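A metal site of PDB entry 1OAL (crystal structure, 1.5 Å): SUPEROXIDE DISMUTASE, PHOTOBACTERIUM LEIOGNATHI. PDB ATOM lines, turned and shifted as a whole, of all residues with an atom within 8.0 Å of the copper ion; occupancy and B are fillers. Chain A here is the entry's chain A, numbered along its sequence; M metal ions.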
ATOM      1  N   GLY A  43     -14.452  11.592  12.065  1.00  0.00           N
ATOM      2  CA  GLY A  43     -15.015  10.256  12.215  1.00  0.00           C
ATOM      3  C   GLY A  43     -16.436  10.230  11.669  1.00  0.00           C
ATOM      4  O   GLY A  43     -17.241  11.175  11.893  1.00  0.00           O
ATOM      5  N   PHE A  44     -16.778   9.103  11.038  1.00  0.00           N
ATOM      6  CA  PHE A  44     -18.015   9.011  10.265  1.00  0.00           C
ATOM      7  C   PHE A  44     -18.488   7.567  10.418  1.00  0.00           C
ATOM      8  O   PHE A  44     -17.833   6.658   9.930  1.00  0.00           O
ATOM      9  CB  PHE A  44     -17.638   9.330   8.803  1.00  0.00           C
ATOM     10  CG  PHE A  44     -18.797   9.458   7.846  1.00  0.00           C
ATOM     11  CD1 PHE A  44     -19.963  10.110   8.187  1.00  0.00           C
ATOM     12  CD2 PHE A  44     -18.666   8.966   6.558  1.00  0.00           C
ATOM     13  CE1 PHE A  44     -21.003  10.262   7.238  1.00  0.00           C
ATOM     14  CE2 PHE A  44     -19.685   9.128   5.626  1.00  0.00           C
ATOM     15  CZ  PHE A  44     -20.852   9.740   5.991  1.00  0.00           C
ATOM     16  N   HIS A  45     -19.622   7.364  11.096  1.00  0.00           N
ATOM     17  CA  HIS A  45     -20.081   5.970  11.354  1.00  0.00           C
ATOM     18  C   HIS A  45     -21.584   5.851  11.358  1.00  0.00           C
ATOM     19  O   HIS A  45     -22.289   6.814  11.627  1.00  0.00           O
ATOM     20  CB  HIS A  45     -19.615   5.420  12.733  1.00  0.00           C
ATOM     21  CG  HIS A  45     -18.337   6.017  13.227  1.00  0.00           C
ATOM     22  ND1 HIS A  45     -18.317   6.947  14.258  1.00  0.00           N
ATOM     23  CD2 HIS A  45     -17.056   5.849  12.833  1.00  0.00           C
ATOM     24  CE1 HIS A  45     -17.058   7.303  14.491  1.00  0.00           C
ATOM     25  NE2 HIS A  45     -16.283   6.688  13.610  1.00  0.00           N
ATOM     26  N   ILE A  46     -22.065   4.652  11.063  1.00  0.00           N
ATOM     27  CA  ILE A  46     -23.479   4.313  11.285  1.00  0.00           C
ATOM     28  C   ILE A  46     -23.572   3.923  12.744  1.00  0.00           C
ATOM     29  O   ILE A  46     -22.744   3.137  13.244  1.00  0.00           O
ATOM     30  CB  ILE A  46     -23.890   3.116  10.426  1.00  0.00           C
ATOM     31  CG1 ILE A  46     -23.538   3.321   8.965  1.00  0.00           C
ATOM     32  CG2 ILE A  46     -25.408   2.825  10.604  1.00  0.00           C
ATOM     33  CD1 ILE A  46     -24.174   4.570   8.333  1.00  0.00           C
ATOM     34  N   HIS A  47     -24.550   4.480  13.430  1.00  0.00           N
ATOM     35  CA  HIS A  47     -24.840   4.107  14.832  1.00  0.00           C
ATOM     36  C   HIS A  47     -26.118   3.292  14.922  1.00  0.00           C
ATOM     37  O   HIS A  47     -26.945   3.253  13.971  1.00  0.00           O
ATOM     38  CB  HIS A  47     -24.935   5.364  15.718  1.00  0.00           C
ATOM     39  CG  HIS A  47     -23.604   5.979  15.997  1.00  0.00           C
ATOM     40  ND1 HIS A  47     -23.136   6.177  17.270  1.00  0.00           N
ATOM     41  CD2 HIS A  47     -22.628   6.417  15.161  1.00  0.00           C
ATOM     42  CE1 HIS A  47     -21.929   6.720  17.211  1.00  0.00           C
ATOM     43  NE2 HIS A  47     -21.595   6.861  15.939  1.00  0.00           N
ATOM     44  N   ALA A  67     -28.523   7.908  19.727  1.00  0.00           N
ATOM     45  CA  ALA A  67     -28.201   7.022  18.616  1.00  0.00           C
ATOM     46  C   ALA A  67     -27.492   5.778  19.088  1.00  0.00           C
ATOM     47  O   ALA A  67     -27.307   4.824  18.329  1.00  0.00           O
ATOM     48  CB  ALA A  67     -27.347   7.773  17.579  1.00  0.00           C
ATOM     49  N   GLY A  68     -27.090   5.745  20.361  1.00  0.00           N
ATOM     50  CA  GLY A  68     -26.329   4.619  20.856  1.00  0.00           C
ATOM     51  C   GLY A  68     -24.936   4.499  20.233  1.00  0.00           C
ATOM     52  O   GLY A  68     -24.344   5.494  19.742  1.00  0.00           O
ATOM     53  N   GLY A  69     -24.424   3.279  20.246  1.00  0.00           N
ATOM     54  CA  GLY A  69     -23.052   3.000  19.832  1.00  0.00           C
ATOM     55  C   GLY A  69     -22.946   2.768  18.342  1.00  0.00           C
ATOM     56  O   GLY A  69     -23.933   2.912  17.604  1.00  0.00           O
ATOM     57  N   HIS A  70     -21.763   2.386  17.896  1.00  0.00           N
ATOM     58  CA  HIS A  70     -21.589   2.040  16.484  1.00  0.00           C
ATOM     59  C   HIS A  70     -22.406   0.807  16.092  1.00  0.00           C
ATOM     60  O   HIS A  70     -22.504  -0.201  16.871  1.00  0.00           O
ATOM     61  CB  HIS A  70     -20.095   1.824  16.159  1.00  0.00           C
ATOM     62  CG  HIS A  70     -19.264   3.069  16.329  1.00  0.00           C
ATOM     63  ND1 HIS A  70     -17.952   3.131  15.906  1.00  0.00           N
ATOM     64  CD2 HIS A  70     -19.536   4.261  16.912  1.00  0.00           C
ATOM     65  CE1 HIS A  70     -17.451   4.327  16.192  1.00  0.00           C
ATOM     66  NE2 HIS A  70     -18.399   5.029  16.806  1.00  0.00           N
ATOM     67  N   TYR A  71     -23.003   0.848  14.893  1.00  0.00           N
ATOM     68  CA  TYR A  71     -23.767  -0.288  14.382  1.00  0.00           C
ATOM     69  C   TYR A  71     -22.848  -1.514  14.302  1.00  0.00           C
ATOM     70  O   TYR A  71     -21.769  -1.457  13.727  1.00  0.00           O
ATOM     71  CB  TYR A  71     -24.283   0.116  12.994  1.00  0.00           C
ATOM     72  CG  TYR A  71     -24.970  -0.969  12.211  1.00  0.00           C
ATOM     73  CD1 TYR A  71     -26.083  -1.649  12.741  1.00  0.00           C
ATOM     74  CD2 TYR A  71     -24.538  -1.325  10.944  1.00  0.00           C
ATOM     75  CE1 TYR A  71     -26.743  -2.640  12.012  1.00  0.00           C
ATOM     76  CE2 TYR A  71     -25.201  -2.343  10.198  1.00  0.00           C
ATOM     77  CZ  TYR A  71     -26.298  -2.982  10.756  1.00  0.00           C
ATOM     78  OH  TYR A  71     -26.953  -3.950  10.019  1.00  0.00           O
ATOM     79  N   HIS A  79     -13.723  -1.408  17.353  1.00  0.00           N
ATOM     80  CA  HIS A  79     -13.744  -0.381  16.296  1.00  0.00           C
ATOM     81  C   HIS A  79     -12.568  -0.609  15.335  1.00  0.00           C
ATOM     82  O   HIS A  79     -11.462  -0.942  15.748  1.00  0.00           O
ATOM     83  CB  HIS A  79     -13.673   1.006  16.911  1.00  0.00           C
ATOM     84  CG  HIS A  79     -13.730   2.098  15.892  1.00  0.00           C
ATOM     85  ND1 HIS A  79     -14.881   2.409  15.183  1.00  0.00           N
ATOM     86  CD2 HIS A  79     -12.758   2.928  15.421  1.00  0.00           C
ATOM     87  CE1 HIS A  79     -14.608   3.394  14.327  1.00  0.00           C
ATOM     88  NE2 HIS A  79     -13.323   3.721  14.451  1.00  0.00           N
ATOM     89  N   HIS A  88     -16.965  -3.100  14.123  1.00  0.00           N
ATOM     90  CA  HIS A  88     -18.338  -2.597  13.835  1.00  0.00           C
ATOM     91  C   HIS A  88     -18.598  -2.498  12.307  1.00  0.00           C
ATOM     92  O   HIS A  88     -17.840  -1.869  11.585  1.00  0.00           O
ATOM     93  CB  HIS A  88     -18.570  -1.206  14.409  1.00  0.00           C
ATOM     94  CG  HIS A  88     -18.111  -1.036  15.815  1.00  0.00           C
ATOM     95  ND1 HIS A  88     -17.315   0.017  16.207  1.00  0.00           N
ATOM     96  CD2 HIS A  88     -18.363  -1.767  16.921  1.00  0.00           C
ATOM     97  CE1 HIS A  88     -17.112  -0.062  17.521  1.00  0.00           C
ATOM     98  NE2 HIS A  88     -17.741  -1.143  17.978  1.00  0.00           N
ATOM     99  N   GLY A  90     -20.673  -0.689  11.141  1.00  0.00           N
ATOM    100  CA  GLY A  90     -20.927   0.742  10.922  1.00  0.00           C
ATOM    101  C   GLY A  90     -19.711   1.627  10.679  1.00  0.00           C
ATOM    102  O   GLY A  90     -19.851   2.861  10.544  1.00  0.00           O
ATOM    103  N   ASP A  91     -18.527   1.040  10.666  1.00  0.00           N
ATOM    104  CA  ASP A  91     -17.296   1.840  10.535  1.00  0.00           C
ATOM    105  C   ASP A  91     -17.065   2.272   9.075  1.00  0.00           C
ATOM    106  O   ASP A  91     -16.728   1.448   8.238  1.00  0.00           O
ATOM    107  CB  ASP A  91     -16.109   1.049  11.057  1.00  0.00           C
ATOM    108  CG  ASP A  91     -16.209   0.811  12.530  1.00  0.00           C
ATOM    109  OD1 ASP A  91     -16.962   1.540  13.202  1.00  0.00           O
ATOM    110  OD2 ASP A  91     -15.491  -0.044  13.119  1.00  0.00           O
ATOM    111  N   ALA A 121     -28.746   5.574  12.394  1.00  0.00           N
ATOM    112  CA  ALA A 121     -28.323   6.957  12.314  1.00  0.00           C
ATOM    113  C   ALA A 121     -26.941   7.060  11.692  1.00  0.00           C
ATOM    114  O   ALA A 121     -26.122   6.168  11.843  1.00  0.00           O
ATOM    115  CB  ALA A 121     -28.345   7.610  13.672  1.00  0.00           C
ATOM    116  N   ILE A 122     -26.708   8.133  10.949  1.00  0.00           N
ATOM    117  CA  ILE A 122     -25.390   8.491  10.455  1.00  0.00           C
ATOM    118  C   ILE A 122     -24.825   9.579  11.358  1.00  0.00           C
ATOM    119  O   ILE A 122     -25.468  10.580  11.614  1.00  0.00           O
ATOM    120  CB  ILE A 122     -25.464   9.074   9.049  1.00  0.00           C
ATOM    121  CG1 ILE A 122     -26.074   8.079   8.076  1.00  0.00           C
ATOM    122  CG2 ILE A 122     -24.020   9.501   8.623  1.00  0.00           C
ATOM    123  CD1 ILE A 122     -26.171   8.607   6.623  1.00  0.00           C
ATOM    124  N   MET A 123     -23.615   9.367  11.836  1.00  0.00           N
ATOM    125  CA  MET A 123     -22.978  10.288  12.738  1.00  0.00           C
ATOM    126  C   MET A 123     -21.686  10.870  12.193  1.00  0.00           C
ATOM    127  O   MET A 123     -20.868  10.125  11.639  1.00  0.00           O
ATOM    128  CB  MET A 123     -22.645   9.557  14.063  1.00  0.00           C
ATOM    129  CG  MET A 123     -22.487  10.543  15.262  1.00  0.00           C
ATOM    130  SD  MET A 123     -24.089  11.240  15.779  1.00  0.00           S
ATOM    131  CE  MET A 123     -24.938   9.735  16.306  1.00  0.00           C
ATOM    132  N   ILE A 124     -21.470  12.168  12.418  1.00  0.00           N
ATOM    133  CA  ILE A 124     -20.195  12.815  12.135  1.00  0.00           C
ATOM    134  C   ILE A 124     -19.654  13.330  13.444  1.00  0.00           C
ATOM    135  O   ILE A 124     -20.402  13.933  14.230  1.00  0.00           O
ATOM    136  CB  ILE A 124     -20.381  13.985  11.144  1.00  0.00           C
ATOM    137  CG1 ILE A 124     -20.905  13.439   9.809  1.00  0.00           C
ATOM    138  CG2 ILE A 124     -19.066  14.740  10.963  1.00  0.00           C
ATOM    139  CD1 ILE A 124     -21.374  14.559   8.855  1.00  0.00           C
ATOM    140  N   HIS A 125     -18.398  13.023  13.722  1.00  0.00           N
ATOM    141  CA  HIS A 125     -17.794  13.380  15.011  1.00  0.00           C
ATOM    142  C   HIS A 125     -16.869  14.581  14.907  1.00  0.00           C
ATOM    143  O   HIS A 125     -16.484  14.992  13.805  1.00  0.00           O
ATOM    144  CB  HIS A 125     -17.009  12.170  15.573  1.00  0.00           C
ATOM    145  CG  HIS A 125     -17.885  11.019  15.953  1.00  0.00           C
ATOM    146  ND1 HIS A 125     -18.223  10.735  17.267  1.00  0.00           N
ATOM    147  CD2 HIS A 125     -18.502  10.089  15.196  1.00  0.00           C
ATOM    148  CE1 HIS A 125     -19.018   9.670  17.290  1.00  0.00           C
ATOM    149  NE2 HIS A 125     -19.183   9.240  16.048  1.00  0.00           N
ATOM    150  N   ASP A 129     -10.655   9.710  12.776  1.00  0.00           N
ATOM    151  CA  ASP A 129     -10.872   8.279  12.933  1.00  0.00           C
ATOM    152  C   ASP A 129      -9.643   7.505  12.494  1.00  0.00           C
ATOM    153  O   ASP A 129      -9.354   7.392  11.303  1.00  0.00           O
ATOM    154  CB  ASP A 129     -12.106   7.820  12.133  1.00  0.00           C
ATOM    155  CG  ASP A 129     -12.588   6.437  12.553  1.00  0.00           C
ATOM    156  OD1 ASP A 129     -11.840   5.668  13.221  1.00  0.00           O
ATOM    157  OD2 ASP A 129     -13.681   6.023  12.193  1.00  0.00           O
ATOM    158  N   LEU A 138     -12.884   4.304  19.938  1.00  0.00           N
ATOM    159  CA  LEU A 138     -13.767   4.657  18.816  1.00  0.00           C
ATOM    160  C   LEU A 138     -13.083   5.579  17.801  1.00  0.00           C
ATOM    161  O   LEU A 138     -13.723   6.456  17.201  1.00  0.00           O
ATOM    162  CB  LEU A 138     -15.063   5.248  19.346  1.00  0.00           C
ATOM    163  CG  LEU A 138     -15.810   4.270  20.292  1.00  0.00           C
ATOM    164  CD1 LEU A 138     -16.942   5.003  21.003  1.00  0.00           C
ATOM    165  CD2 LEU A 138     -16.330   3.023  19.497  1.00  0.00           C
ATOM    166  N   GLY A 141     -12.905   9.829  17.576  1.00  0.00           N
ATOM    167  CA  GLY A 141     -13.936  10.753  17.097  1.00  0.00           C
ATOM    168  C   GLY A 141     -14.429  11.712  18.160  1.00  0.00           C
ATOM    169  O   GLY A 141     -14.829  12.872  17.873  1.00  0.00           O
ATOM    170  N   GLY A 142     -14.494  11.231  19.391  1.00  0.00           N
ATOM    171  CA  GLY A 142     -14.992  12.069  20.459  1.00  0.00           C
ATOM    172  C   GLY A 142     -16.425  12.506  20.235  1.00  0.00           C
ATOM    173  O   GLY A 142     -17.317  11.681  19.918  1.00  0.00           O
ATOM    174  N   ALA A 143     -16.691  13.785  20.503  1.00  0.00           N
ATOM    175  CA  ALA A 143     -18.052  14.283  20.497  1.00  0.00           C
ATOM    176  C   ALA A 143     -18.745  14.114  19.158  1.00  0.00           C
ATOM    177  O   ALA A 143     -18.098  14.116  18.096  1.00  0.00           O
ATOM    178  CB  ALA A 143     -18.081  15.765  20.918  1.00  0.00           C
ATOM    179  N   ARG A 144     -20.072  13.986  19.215  1.00  0.00           N
ATOM    180  CA  ARG A 144     -20.886  13.908  18.025  1.00  0.00           C
ATOM    181  C   ARG A 144     -21.251  15.335  17.624  1.00  0.00           C
ATOM    182  O   ARG A 144     -21.779  16.119  18.444  1.00  0.00           O
ATOM    183  CB  ARG A 144     -22.125  13.067  18.329  1.00  0.00           C
ATOM    184  CG  ARG A 144     -21.770  11.649  18.748  1.00  0.00           C
ATOM    185  CD  ARG A 144     -22.884  10.864  19.468  1.00  0.00           C
ATOM    186  NE  ARG A 144     -22.309   9.631  20.012  1.00  0.00           N
ATOM    187  CZ  ARG A 144     -22.963   8.496  20.212  1.00  0.00           C
ATOM    188  NH1 ARG A 144     -24.251   8.358  19.912  1.00  0.00           N
ATOM    189  NH2 ARG A 144     -22.285   7.447  20.655  1.00  0.00           N
ATOM    190  N   ALA A 146     -22.707  16.158  14.138  1.00  0.00           N
ATOM    191  CA  ALA A 146     -23.822  16.221  13.201  1.00  0.00           C
ATOM    192  C   ALA A 146     -24.392  14.824  13.031  1.00  0.00           C
ATOM    193  O   ALA A 146     -23.681  13.833  13.192  1.00  0.00           O
ATOM    194  CB  ALA A 146     -23.392  16.833  11.835  1.00  0.00           C
HETATM  195 CU    CU M   1     -19.842   7.479  15.387  1.00  0.00          CU
HETATM  196 ZN    ZN M   2     -16.773   1.631  15.173  1.00  0.00          ZN
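A ring nitrogen (ND1) of His 47 lies close to the backbone carbonyl oxygen of Gly 69, at 3.4 Å. A ring nitrogen (ND1) of His 47 lies within hydrogen-bond range of the backbone carbonyl oxygen (O) of Gly 68, at 2.8 Å. O of Ala 121 sits at hydrogen-bond distance from N of His 47. A ring nitrogen (ND1) of His 45 sits close to a ring nitrogen (NE2) of His 70 (3.2 Å). The backbone NH (N) of Met 123 sits at hydrogen-bond distance from the backbone carbonyl oxygen (O) of His 45 (2.9 Å). A ring nitrogen (NE2) of His 45 is in hydrogen-bond range of the side-chain carboxylate of Asp 129, 3.0 Å away. O of Gly 142 sits at hydrogen-bond distance from ND1 of His 125 (3.0 Å). O of Ala 143 sits close to ND1 of His 125 (3.5 Å).
Merely in contact with the copper ion: His 70 (3.2 Å) and Met 123 (3.7 Å). Within 4 Å of the copper ion: His 45, His 47, His 70, Met 123 and His 125. The nearest printed residue that does not touch the copper ion is Phe 44 (5.2 Å).
The copper ion is bound by a ring nitrogen (NE2) of His 47, a ring nitrogen (ND1) of His 45 and a ring nitrogen (NE2) of His 125.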
